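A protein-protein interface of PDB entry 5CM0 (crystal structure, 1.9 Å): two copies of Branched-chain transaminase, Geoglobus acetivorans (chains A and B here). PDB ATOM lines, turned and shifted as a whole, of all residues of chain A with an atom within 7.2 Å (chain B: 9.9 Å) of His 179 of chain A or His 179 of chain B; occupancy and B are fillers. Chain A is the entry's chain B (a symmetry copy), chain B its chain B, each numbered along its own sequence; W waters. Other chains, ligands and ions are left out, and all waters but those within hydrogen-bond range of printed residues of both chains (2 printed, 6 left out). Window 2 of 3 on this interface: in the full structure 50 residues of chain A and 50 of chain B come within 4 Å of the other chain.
The backbone carbonyl oxygen (O) of Asp 145 of chain B sits at hydrogen-bond distance from the backbone NH (N) of Arg 140 of chain A. O of Asp 145 of chain A is in hydrogen-bond range of N of Arg 140 of chain B.
NE of Arg 140 of chain A is in hydrogen-bond range of O of Asp 178 of chain A (3.3 Å). The backbone NH of Arg 141 of chain A lies within hydrogen-bond range of the backbone carbonyl oxygen of Leu 177 of chain A (2.9 Å). OG of Ser 146 of chain B lies close to O of Ala 143 of chain B (3.2 Å). ND2 of Asn 158 of chain B sits at hydrogen-bond distance from O of Arg 140 of chain B, at 3.0 Å. NE of Arg 140 of chain B sits at hydrogen-bond distance from O of Asp 178 of chain B (3.3 Å).
Among the printed residues, merely in contact across the chains: Arg 140 of chain A with Ser 146 of chain B (3.2 Å), Asp 145 of chain A with Ile 139 of chain B (3.3 Å), His 179 of chain A with His 179 of chain B (3.5 Å) and Arg 141 of chain A with Ser 146 of chain B (3.9 Å).
Of the printed residues of chain B, Arg 141 of chain A touches Ser 146 (3.9 Å). Printed residues of chain B within 4 Å of Asp 145 of chain A: Ile 139 (3.3 Å) and Arg 140 (2.7 Å). His 179 of chain A touches just one residue of chain B: His 179. No residue of chain B comes within 4 Å of Asn 180 of chain A. Of the printed residues of chain A, Ser 146 of chain B touches Arg 140 and Arg 141. Asn 158 of chain B touches none of the printed residues of chain A. His 179 of chain B touches just one residue of chain A: His 179 (3.5 Å). Ile 183 of chain B touches none of the printed residues of chain A. The nearest residue of chain B that does not touch His 179 of chain A is Asp 145 of chain B (4.8 Å). The nearest printed residue of chain B that does not touch Arg 140 of chain A is Ala 143 of chain B (6.8 Å).
Of the 24 printed residues of chain B, 5 touch a printed residue of chain A. Printed residues of chain B that touch a printed residue of chain A: Ile 139, Arg 140, Asp 145, Ser 146 and His 179. Hydrophobic or aromatic side chains of chain B within 4 Å of the printed part of chain A: Ile 139 and His 179. Along chain B the printed residues that touch a printed residue of chain A span positions 139 to 179. Among the printed residues, no Asp or Glu carboxylate lies within 4 Å of a Lys or Arg side-chain nitrogen of the other chain.
Arg 140 of chain A touches Asp 145 of chain B, and with the chains exchanged Asp 145 of chain A touches Arg 140 of chain B. His 179 of chain A touches its own counterpart, His 179 of chain B. Positions printed for both chains: 140, 141, 142, 143, 145, 177, 178, 179, 180, 181, 182 and 206. Of the 6 pairs that touch across the chains among the printed residues, 3 have their exchanged pair printed and touching as well.
Water W2 bridges the side-chain carboxylate of Asp 145 of chain B (2.6 Å) and a ring nitrogen (ND1) of His 179 of chain A (2.8 Å). Water W1 lies within hydrogen-bond range of OD1 of Asp 145 of chain A (2.6 Å) and ND1 of His 179 of chain B (2.8 Å).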
ATOM      1  N   ARG A 140     -25.601  29.990  14.239  1.00  0.00           N
ATOM      2  CA  ARG A 140     -25.190  30.207  12.879  1.00  0.00           C
ATOM      3  C   ARG A 140     -26.415  30.391  11.951  1.00  0.00           C
ATOM      4  O   ARG A 140     -27.494  30.006  12.312  1.00  0.00           O
ATOM      5  CB  ARG A 140     -24.364  29.011  12.363  1.00  0.00           C
ATOM      6  CG  ARG A 140     -23.052  28.858  13.104  1.00  0.00           C
ATOM      7  CD  ARG A 140     -22.164  30.112  12.952  1.00  0.00           C
ATOM      8  NE  ARG A 140     -20.772  29.939  13.361  1.00  0.00           N
ATOM      9  CZ  ARG A 140     -20.177  30.553  14.371  1.00  0.00           C
ATOM     10  NH1 ARG A 140     -20.796  31.449  15.133  1.00  0.00           N
ATOM     11  NH2 ARG A 140     -18.899  30.304  14.601  1.00  0.00           N
ATOM     12  N   ARG A 141     -26.208  31.050  10.833  1.00  0.00           N
ATOM     13  CA  ARG A 141     -27.244  31.236   9.824  1.00  0.00           C
ATOM     14  C   ARG A 141     -27.765  29.860   9.348  1.00  0.00           C
ATOM     15  O   ARG A 141     -26.975  28.954   9.130  1.00  0.00           O
ATOM     16  CB  ARG A 141     -26.708  31.966   8.624  1.00  0.00           C
ATOM     17  CG  ARG A 141     -27.796  32.611   7.774  1.00  0.00           C
ATOM     18  CD  ARG A 141     -28.539  33.732   8.486  1.00  0.00           C
ATOM     19  NE  ARG A 141     -29.494  34.356   7.567  1.00  0.00           N
ATOM     20  CZ  ARG A 141     -30.741  33.966   7.360  1.00  0.00           C
ATOM     21  NH1 ARG A 141     -31.308  32.942   8.005  1.00  0.00           N
ATOM     22  NH2 ARG A 141     -31.448  34.612   6.450  1.00  0.00           N
ATOM     23  N   ASN A 142     -29.070  29.772   9.111  1.00  0.00           N
ATOM     24  CA  ASN A 142     -29.663  28.616   8.428  1.00  0.00           C
ATOM     25  C   ASN A 142     -28.796  28.212   7.231  1.00  0.00           C
ATOM     26  O   ASN A 142     -28.371  29.043   6.421  1.00  0.00           O
ATOM     27  CB  ASN A 142     -31.046  28.934   7.873  1.00  0.00           C
ATOM     28  CG  ASN A 142     -32.136  28.918   8.919  1.00  0.00           C
ATOM     29  OD1 ASN A 142     -33.182  29.589   8.770  1.00  0.00           O
ATOM     30  ND2 ASN A 142     -31.896  28.214   9.956  1.00  0.00           N
ATOM     31  N   ALA A 143     -28.544  26.906   7.084  1.00  0.00           N
ATOM     32  CA  ALA A 143     -27.565  26.454   6.035  1.00  0.00           C
ATOM     33  C   ALA A 143     -28.166  26.398   4.635  1.00  0.00           C
ATOM     34  O   ALA A 143     -29.390  26.107   4.483  1.00  0.00           O
ATOM     35  CB  ALA A 143     -26.999  25.066   6.397  1.00  0.00           C
ATOM     36  N   ASP A 145     -28.070  24.208   2.476  1.00  0.00           N
ATOM     37  CA  ASP A 145     -28.760  22.929   2.115  1.00  0.00           C
ATOM     38  C   ASP A 145     -29.658  22.332   3.168  1.00  0.00           C
ATOM     39  O   ASP A 145     -29.889  21.125   3.148  1.00  0.00           O
ATOM     40  CB  ASP A 145     -27.762  21.879   1.641  1.00  0.00           C
ATOM     41  CG  ASP A 145     -26.743  21.510   2.728  1.00  0.00           C
ATOM     42  OD1 ASP A 145     -26.724  22.231   3.730  1.00  0.00           O
ATOM     43  OD2 ASP A 145     -26.018  20.515   2.580  1.00  0.00           O
ATOM     44  N   LEU A 177     -22.584  34.430  11.543  1.00  0.00           N
ATOM     45  CA  LEU A 177     -21.680  33.709  10.742  1.00  0.00           C
ATOM     46  C   LEU A 177     -22.432  32.482  10.165  1.00  0.00           C
ATOM     47  O   LEU A 177     -23.505  32.108  10.668  1.00  0.00           O
ATOM     48  CB  LEU A 177     -20.474  33.168  11.585  1.00  0.00           C
ATOM     49  CG  LEU A 177     -19.314  34.201  11.843  1.00  0.00           C
ATOM     50  CD1 LEU A 177     -19.768  35.407  12.594  1.00  0.00           C
ATOM     51  CD2 LEU A 177     -18.240  33.563  12.722  1.00  0.00           C
ATOM     52  N   ASP A 178     -21.845  31.870   9.157  1.00  0.00           N
ATOM     53  CA  ASP A 178     -22.325  30.596   8.680  1.00  0.00           C
ATOM     54  C   ASP A 178     -21.496  29.476   9.275  1.00  0.00           C
ATOM     55  O   ASP A 178     -20.576  29.688  10.087  1.00  0.00           O
ATOM     56  CB  ASP A 178     -22.391  30.541   7.123  1.00  0.00           C
ATOM     57  CG  ASP A 178     -21.046  30.389   6.436  1.00  0.00           C
ATOM     58  OD1 ASP A 178     -19.980  30.158   7.031  1.00  0.00           O
ATOM     59  OD2 ASP A 178     -21.096  30.429   5.202  1.00  0.00           O
ATOM     60  N   HIS A 179     -21.793  28.261   8.805  1.00  0.00           N
ATOM     61  CA  HIS A 179     -21.130  27.064   9.385  1.00  0.00           C
ATOM     62  C   HIS A 179     -19.649  27.024   9.093  1.00  0.00           C
ATOM     63  O   HIS A 179     -18.888  26.462   9.857  1.00  0.00           O
ATOM     64  CB  HIS A 179     -21.810  25.784   8.853  1.00  0.00           C
ATOM     65  CG  HIS A 179     -21.251  24.507   9.452  1.00  0.00           C
ATOM     66  ND1 HIS A 179     -21.521  24.104  10.739  1.00  0.00           N
ATOM     67  CD2 HIS A 179     -20.403  23.574   8.953  1.00  0.00           C
ATOM     68  CE1 HIS A 179     -20.911  22.952  10.994  1.00  0.00           C
ATOM     69  NE2 HIS A 179     -20.219  22.614   9.932  1.00  0.00           N
ATOM     70  N   ASN A 180     -19.263  27.604   7.990  1.00  0.00           N
ATOM     71  CA  ASN A 180     -17.816  27.723   7.597  1.00  0.00           C
ATOM     72  C   ASN A 180     -17.061  28.787   8.363  1.00  0.00           C
ATOM     73  O   ASN A 180     -15.824  28.835   8.276  1.00  0.00           O
ATOM     74  CB  ASN A 180     -17.671  28.058   6.125  1.00  0.00           C
ATOM     75  CG  ASN A 180     -18.457  27.122   5.211  1.00  0.00           C
ATOM     76  OD1 ASN A 180     -18.266  25.898   5.298  1.00  0.00           O
ATOM     77  ND2 ASN A 180     -19.450  27.690   4.425  1.00  0.00           N
ATOM     78  N   GLY A 181     -17.758  29.582   9.147  1.00  0.00           N
ATOM     79  CA  GLY A 181     -17.098  30.704   9.859  1.00  0.00           C
ATOM     80  C   GLY A 181     -17.043  31.968   9.001  1.00  0.00           C
ATOM     81  O   GLY A 181     -16.402  32.964   9.389  1.00  0.00           O
ATOM     82  N   TYR A 182     -17.750  31.976   7.867  1.00  0.00           N
ATOM     83  CA  TYR A 182     -17.814  33.179   7.016  1.00  0.00           C
ATOM     84  C   TYR A 182     -18.887  34.087   7.594  1.00  0.00           C
ATOM     85  O   TYR A 182     -19.926  33.622   8.055  1.00  0.00           O
ATOM     86  CB  TYR A 182     -18.234  32.859   5.572  1.00  0.00           C
ATOM     87  CG  TYR A 182     -17.418  31.876   4.784  1.00  0.00           C
ATOM     88  CD1 TYR A 182     -16.073  31.756   4.963  1.00  0.00           C
ATOM     89  CD2 TYR A 182     -18.040  31.042   3.784  1.00  0.00           C
ATOM     90  CE1 TYR A 182     -15.311  30.850   4.225  1.00  0.00           C
ATOM     91  CE2 TYR A 182     -17.281  30.139   3.030  1.00  0.00           C
ATOM     92  CZ  TYR A 182     -15.900  30.057   3.255  1.00  0.00           C
ATOM     93  OH  TYR A 182     -15.077  29.155   2.621  1.00  0.00           O
ATOM     94  N   ASN A 206     -24.806  32.600   1.211  1.00  0.00           N
ATOM     95  CA  ASN A 206     -25.060  32.266   2.625  1.00  0.00           C
ATOM     96  C   ASN A 206     -25.962  33.215   3.374  1.00  0.00           C
ATOM     97  O   ASN A 206     -26.218  33.015   4.588  1.00  0.00           O
ATOM     98  CB  ASN A 206     -23.759  32.015   3.370  1.00  0.00           C
ATOM     99  CG  ASN A 206     -23.057  33.321   3.800  1.00  0.00           C
ATOM    100  OD1 ASN A 206     -23.601  34.409   3.613  1.00  0.00           O
ATOM    101  ND2 ASN A 206     -21.870  33.194   4.408  1.00  0.00           N
ATOM    102  N   VAL B 137     -33.327  12.235   1.318  1.00  0.00           N
ATOM    103  CA  VAL B 137     -33.484  13.535   0.651  1.00  0.00           C
ATOM    104  C   VAL B 137     -32.163  14.228   0.504  1.00  0.00           C
ATOM    105  O   VAL B 137     -31.237  13.950   1.262  1.00  0.00           O
ATOM    106  CB  VAL B 137     -34.510  14.447   1.307  1.00  0.00           C
ATOM    107  CG1 VAL B 137     -35.909  13.912   1.097  1.00  0.00           C
ATOM    108  CG2 VAL B 137     -34.264  14.675   2.801  1.00  0.00           C
ATOM    109  N   ALA B 138     -32.073  15.121  -0.484  1.00  0.00           N
ATOM    110  CA  ALA B 138     -30.839  15.904  -0.691  1.00  0.00           C
ATOM    111  C   ALA B 138     -30.677  16.973   0.398  1.00  0.00           C
ATOM    112  O   ALA B 138     -29.582  17.211   0.863  1.00  0.00           O
ATOM    113  CB  ALA B 138     -30.876  16.548  -2.038  1.00  0.00           C
ATOM    114  N   ILE B 139     -31.775  17.587   0.813  1.00  0.00           N
ATOM    115  CA  ILE B 139     -31.759  18.580   1.886  1.00  0.00           C
ATOM    116  C   ILE B 139     -31.376  17.949   3.229  1.00  0.00           C
ATOM    117  O   ILE B 139     -31.865  16.856   3.568  1.00  0.00           O
ATOM    118  CB  ILE B 139     -33.147  19.292   1.889  1.00  0.00           C
ATOM    119  CG1 ILE B 139     -33.110  20.615   2.608  1.00  0.00           C
ATOM    120  CG2 ILE B 139     -34.300  18.496   2.468  1.00  0.00           C
ATOM    121  CD1 ILE B 139     -32.994  21.705   1.598  1.00  0.00           C
ATOM    122  N   ARG B 140     -30.539  18.618   4.019  1.00  0.00           N
ATOM    123  CA  ARG B 140     -30.140  18.116   5.305  1.00  0.00           C
ATOM    124  C   ARG B 140     -31.044  18.682   6.426  1.00  0.00           C
ATOM    125  O   ARG B 140     -31.689  19.675   6.222  1.00  0.00           O
ATOM    126  CB  ARG B 140     -28.681  18.506   5.613  1.00  0.00           C
ATOM    127  CG  ARG B 140     -27.699  17.850   4.663  1.00  0.00           C
ATOM    128  CD  ARG B 140     -27.775  16.310   4.741  1.00  0.00           C
ATOM    129  NE  ARG B 140     -26.667  15.603   4.105  1.00  0.00           N
ATOM    130  CZ  ARG B 140     -26.755  14.810   3.049  1.00  0.00           C
ATOM    131  NH1 ARG B 140     -27.910  14.539   2.448  1.00  0.00           N
ATOM    132  NH2 ARG B 140     -25.659  14.222   2.603  1.00  0.00           N
ATOM    133  N   ARG B 141     -31.116  17.976   7.532  1.00  0.00           N
ATOM    134  CA  ARG B 141     -31.864  18.418   8.704  1.00  0.00           C
ATOM    135  C   ARG B 141     -31.330  19.789   9.179  1.00  0.00           C
ATOM    136  O   ARG B 141     -30.126  19.992   9.215  1.00  0.00           O
ATOM    137  CB  ARG B 141     -31.715  17.446   9.840  1.00  0.00           C
ATOM    138  CG  ARG B 141     -32.813  17.572  10.890  1.00  0.00           C
ATOM    139  CD  ARG B 141     -34.194  17.199  10.371  1.00  0.00           C
ATOM    140  NE  ARG B 141     -35.167  17.255  11.465  1.00  0.00           N
ATOM    141  CZ  ARG B 141     -35.846  18.324  11.848  1.00  0.00           C
ATOM    142  NH1 ARG B 141     -35.746  19.512  11.245  1.00  0.00           N
ATOM    143  NH2 ARG B 141     -36.643  18.208  12.895  1.00  0.00           N
ATOM    144  N   ASN B 142     -32.237  20.657   9.617  1.00  0.00           N
ATOM    145  CA  ASN B 142     -31.862  21.890  10.319  1.00  0.00           C
ATOM    146  C   ASN B 142     -30.754  21.598  11.336  1.00  0.00           C
ATOM    147  O   ASN B 142     -30.816  20.639  12.113  1.00  0.00           O
ATOM    148  CB  ASN B 142     -33.030  22.470  11.106  1.00  0.00           C
ATOM    149  CG  ASN B 142     -34.023  23.221  10.250  1.00  0.00           C
ATOM    150  OD1 ASN B 142     -35.218  23.340  10.602  1.00  0.00           O
ATOM    151  ND2 ASN B 142     -33.568  23.680   9.150  1.00  0.00           N
ATOM    152  N   ALA B 143     -29.724  22.452  11.367  1.00  0.00           N
ATOM    153  CA  ALA B 143     -28.524  22.136  12.218  1.00  0.00           C
ATOM    154  C   ALA B 143     -28.725  22.474  13.690  1.00  0.00           C
ATOM    155  O   ALA B 143     -29.457  23.454  14.021  1.00  0.00           O
ATOM    156  CB  ALA B 143     -27.285  22.888  11.692  1.00  0.00           C
ATOM    157  N   ILE B 144     -28.027  21.732  14.566  1.00  0.00           N
ATOM    158  CA  ILE B 144     -28.176  21.917  15.999  1.00  0.00           C
ATOM    159  C   ILE B 144     -27.714  23.306  16.465  1.00  0.00           C
ATOM    160  O   ILE B 144     -28.052  23.694  17.555  1.00  0.00           O
ATOM    161  CB  ILE B 144     -27.473  20.880  16.825  1.00  0.00           C
ATOM    162  CG1 ILE B 144     -25.966  20.896  16.499  1.00  0.00           C
ATOM    163  CG2 ILE B 144     -28.105  19.535  16.572  1.00  0.00           C
ATOM    164  CD1 ILE B 144     -25.194  19.886  17.338  1.00  0.00           C
ATOM    165  N   ASP B 145     -26.941  24.002  15.678  1.00  0.00           N
ATOM    166  CA  ASP B 145     -26.616  25.410  16.072  1.00  0.00           C
ATOM    167  C   ASP B 145     -27.101  26.494  15.146  1.00  0.00           C
ATOM    168  O   ASP B 145     -26.524  27.579  15.134  1.00  0.00           O
ATOM    169  CB  ASP B 145     -25.122  25.581  16.320  1.00  0.00           C
ATOM    170  CG  ASP B 145     -24.286  25.296  15.064  1.00  0.00           C
ATOM    171  OD1 ASP B 145     -24.882  24.778  14.115  1.00  0.00           O
ATOM    172  OD2 ASP B 145     -23.088  25.613  15.037  1.00  0.00           O
ATOM    173  N   SER B 146     -28.139  26.220  14.370  1.00  0.00           N
ATOM    174  CA  SER B 146     -28.836  27.254  13.585  1.00  0.00           C
ATOM    175  C   SER B 146     -30.311  27.304  13.910  1.00  0.00           C
ATOM    176  O   SER B 146     -30.827  28.334  14.268  1.00  0.00           O
ATOM    177  CB  SER B 146     -28.596  27.010  12.092  1.00  0.00           C
ATOM    178  OG  SER B 146     -28.839  25.653  11.758  1.00  0.00           O
ATOM    179  N   PRO B 149     -33.126  21.137  15.901  1.00  0.00           N
ATOM    180  CA  PRO B 149     -34.245  20.297  15.466  1.00  0.00           C
ATOM    181  C   PRO B 149     -35.042  19.790  16.667  1.00  0.00           C
ATOM    182  O   PRO B 149     -36.232  19.440  16.492  1.00  0.00           O
ATOM    183  CB  PRO B 149     -33.566  19.217  14.574  1.00  0.00           C
ATOM    184  CG  PRO B 149     -32.179  19.124  15.141  1.00  0.00           C
ATOM    185  CD  PRO B 149     -31.837  20.531  15.546  1.00  0.00           C
ATOM    186  N   ASN B 158     -38.130  23.238   6.679  1.00  0.00           N
ATOM    187  CA  ASN B 158     -37.073  22.203   6.424  1.00  0.00           C
ATOM    188  C   ASN B 158     -37.769  20.834   6.137  1.00  0.00           C
ATOM    189  O   ASN B 158     -37.469  20.149   5.189  1.00  0.00           O
ATOM    190  CB  ASN B 158     -36.258  22.081   7.691  1.00  0.00           C
ATOM    191  CG  ASN B 158     -35.087  21.081   7.629  1.00  0.00           C
ATOM    192  OD1 ASN B 158     -34.861  20.361   8.595  1.00  0.00           O
ATOM    193  ND2 ASN B 158     -34.311  21.127   6.593  1.00  0.00           N
ATOM    194  N   PHE B 176     -34.055  12.256   6.443  1.00  0.00           N
ATOM    195  CA  PHE B 176     -32.969  13.284   6.501  1.00  0.00           C
ATOM    196  C   PHE B 176     -31.679  12.673   7.012  1.00  0.00           C
ATOM    197  O   PHE B 176     -31.706  11.803   7.883  1.00  0.00           O
ATOM    198  CB  PHE B 176     -33.282  14.316   7.547  1.00  0.00           C
ATOM    199  CG  PHE B 176     -34.286  15.340   7.191  1.00  0.00           C
ATOM    200  CD1 PHE B 176     -33.949  16.400   6.352  1.00  0.00           C
ATOM    201  CD2 PHE B 176     -35.535  15.395   7.884  1.00  0.00           C
ATOM    202  CE1 PHE B 176     -34.846  17.434   6.132  1.00  0.00           C
ATOM    203  CE2 PHE B 176     -36.435  16.423   7.678  1.00  0.00           C
ATOM    204  CZ  PHE B 176     -36.089  17.465   6.836  1.00  0.00           C
ATOM    205  N   LEU B 177     -30.559  13.121   6.442  1.00  0.00           N
ATOM    206  CA  LEU B 177     -29.288  13.076   7.045  1.00  0.00           C
ATOM    207  C   LEU B 177     -29.008  14.469   7.665  1.00  0.00           C
ATOM    208  O   LEU B 177     -29.678  15.457   7.321  1.00  0.00           O
ATOM    209  CB  LEU B 177     -28.163  12.795   5.990  1.00  0.00           C
ATOM    210  CG  LEU B 177     -27.959  11.282   5.608  1.00  0.00           C
ATOM    211  CD1 LEU B 177     -29.178  10.666   5.009  1.00  0.00           C
ATOM    212  CD2 LEU B 177     -26.880  11.161   4.533  1.00  0.00           C
ATOM    213  N   ASP B 178     -28.015  14.525   8.529  1.00  0.00           N
ATOM    214  CA  ASP B 178     -27.514  15.791   9.004  1.00  0.00           C
ATOM    215  C   ASP B 178     -26.277  16.183   8.221  1.00  0.00           C
ATOM    216  O   ASP B 178     -25.835  15.491   7.286  1.00  0.00           O
ATOM    217  CB  ASP B 178     -27.279  15.787  10.546  1.00  0.00           C
ATOM    218  CG  ASP B 178     -26.044  15.029  10.998  1.00  0.00           C
ATOM    219  OD1 ASP B 178     -25.180  14.580  10.227  1.00  0.00           O
ATOM    220  OD2 ASP B 178     -25.909  14.959  12.225  1.00  0.00           O
ATOM    221  N   HIS B 179     -25.673  17.289   8.664  1.00  0.00           N
ATOM    222  CA  HIS B 179     -24.512  17.845   7.918  1.00  0.00           C
ATOM    223  C   HIS B 179     -23.306  16.937   7.965  1.00  0.00           C
ATOM    224  O   HIS B 179     -22.497  16.945   7.058  1.00  0.00           O
ATOM    225  CB  HIS B 179     -24.152  19.237   8.478  1.00  0.00           C
ATOM    226  CG  HIS B 179     -23.025  19.920   7.726  1.00  0.00           C
ATOM    227  ND1 HIS B 179     -23.187  20.475   6.479  1.00  0.00           N
ATOM    228  CD2 HIS B 179     -21.714  20.092   8.029  1.00  0.00           C
ATOM    229  CE1 HIS B 179     -22.044  21.008   6.064  1.00  0.00           C
ATOM    230  NE2 HIS B 179     -21.133  20.782   6.981  1.00  0.00           N
ATOM    231  N   ASN B 180     -23.195  16.181   9.023  1.00  0.00           N
ATOM    232  CA  ASN B 180     -22.097  15.166   9.185  1.00  0.00           C
ATOM    233  C   ASN B 180     -22.304  13.909   8.368  1.00  0.00           C
ATOM    234  O   ASN B 180     -21.373  13.097   8.258  1.00  0.00           O
ATOM    235  CB  ASN B 180     -21.959  14.731  10.631  1.00  0.00           C
ATOM    236  CG  ASN B 180     -21.831  15.899  11.604  1.00  0.00           C
ATOM    237  OD1 ASN B 180     -20.936  16.740  11.419  1.00  0.00           O
ATOM    238  ND2 ASN B 180     -22.819  16.029  12.570  1.00  0.00           N
ATOM    239  N   GLY B 181     -23.459  13.766   7.753  1.00  0.00           N
ATOM    240  CA  GLY B 181     -23.767  12.520   7.009  1.00  0.00           C
ATOM    241  C   GLY B 181     -24.373  11.450   7.917  1.00  0.00           C
ATOM    242  O   GLY B 181     -24.564  10.296   7.488  1.00  0.00           O
ATOM    243  N   TYR B 182     -24.737  11.820   9.149  1.00  0.00           N
ATOM    244  CA  TYR B 182     -25.399  10.872  10.065  1.00  0.00           C
ATOM    245  C   TYR B 182     -26.879  10.864   9.719  1.00  0.00           C
ATOM    246  O   TYR B 182     -27.459  11.900   9.406  1.00  0.00           O
ATOM    247  CB  TYR B 182     -25.289  11.302  11.537  1.00  0.00           C
ATOM    248  CG  TYR B 182     -23.926  11.517  12.128  1.00  0.00           C
ATOM    249  CD1 TYR B 182     -22.849  10.784  11.728  1.00  0.00           C
ATOM    250  CD2 TYR B 182     -23.722  12.498  13.165  1.00  0.00           C
ATOM    251  CE1 TYR B 182     -21.583  10.974  12.282  1.00  0.00           C
ATOM    252  CE2 TYR B 182     -22.458  12.688  13.736  1.00  0.00           C
ATOM    253  CZ  TYR B 182     -21.385  11.905  13.288  1.00  0.00           C
ATOM    254  OH  TYR B 182     -20.091  12.062  13.729  1.00  0.00           O
ATOM    255  N   ILE B 183     -27.497   9.690   9.773  1.00  0.00           N
ATOM    256  CA  ILE B 183     -28.948   9.616   9.695  1.00  0.00           C
ATOM    257  C   ILE B 183     -29.545  10.435  10.867  1.00  0.00           C
ATOM    258  O   ILE B 183     -29.014  10.390  11.984  1.00  0.00           O
ATOM    259  CB  ILE B 183     -29.461   8.147   9.765  1.00  0.00           C
ATOM    260  CG1 ILE B 183     -28.777   7.232   8.707  1.00  0.00           C
ATOM    261  CG2 ILE B 183     -30.979   8.162   9.669  1.00  0.00           C
ATOM    262  CD1 ILE B 183     -28.810   7.687   7.261  1.00  0.00           C
ATOM    263  N   SER B 184     -30.574  11.227  10.557  1.00  0.00           N
ATOM    264  CA  SER B 184     -31.296  12.048  11.515  1.00  0.00           C
ATOM    265  C   SER B 184     -32.649  11.401  11.897  1.00  0.00           C
ATOM    266  O   SER B 184     -32.784  10.845  13.005  1.00  0.00           O
ATOM    267  CB  SER B 184     -31.433  13.473  10.991  1.00  0.00           C
ATOM    268  OG  SER B 184     -32.228  14.266  11.845  1.00  0.00           O
ATOM    269  N   ASN B 206     -29.461  15.348  16.875  1.00  0.00           N
ATOM    270  CA  ASN B 206     -29.675  15.847  15.504  1.00  0.00           C
ATOM    271  C   ASN B 206     -31.077  15.710  14.965  1.00  0.00           C
ATOM    272  O   ASN B 206     -31.344  16.094  13.798  1.00  0.00           O
ATOM    273  CB  ASN B 206     -28.642  15.275  14.548  1.00  0.00           C
ATOM    274  CG  ASN B 206     -28.986  13.843  14.085  1.00  0.00           C
ATOM    275  OD1 ASN B 206     -30.051  13.322  14.418  1.00  0.00           O
ATOM    276  ND2 ASN B 206     -28.096  13.238  13.288  1.00  0.00           N
ATOM    277  N   ASN B 207     -31.996  15.251  15.809  1.00  0.00           N
ATOM    278  CA  ASN B 207     -33.396  15.062  15.392  1.00  0.00           C
ATOM    279  C   ASN B 207     -34.349  15.657  16.442  1.00  0.00           C
ATOM    280  O   ASN B 207     -34.363  16.884  16.645  1.00  0.00           O
ATOM    281  CB  ASN B 207     -33.691  13.575  15.024  1.00  0.00           C
ATOM    282  CG  ASN B 207     -33.192  12.594  16.096  1.00  0.00           C
ATOM    283  OD1 ASN B 207     -33.901  12.281  17.073  1.00  0.00           O
ATOM    284  ND2 ASN B 207     -32.002  12.141  15.947  1.00  0.00           N
ATOM    285  N   ASN B 231     -24.882   6.850  16.437  1.00  0.00           N
ATOM    286  CA  ASN B 231     -24.976   7.317  15.092  1.00  0.00           C
ATOM    287  C   ASN B 231     -24.765   6.299  14.064  1.00  0.00           C
ATOM    288  O   ASN B 231     -23.900   5.434  14.213  1.00  0.00           O
ATOM    289  CB  ASN B 231     -24.062   8.516  14.876  1.00  0.00           C
ATOM    290  CG  ASN B 231     -24.682   9.822  15.540  1.00  0.00           C
ATOM    291  OD1 ASN B 231     -25.861  10.259  15.325  1.00  0.00           O
ATOM    292  ND2 ASN B 231     -23.911  10.380  16.318  1.00  0.00           N
HETATM  293  O   HOH W   1     -25.851  20.646   5.645  1.00  0.00           O
HETATM  294  O   HOH W   2     -23.534  25.581  11.998  1.00  0.00           O
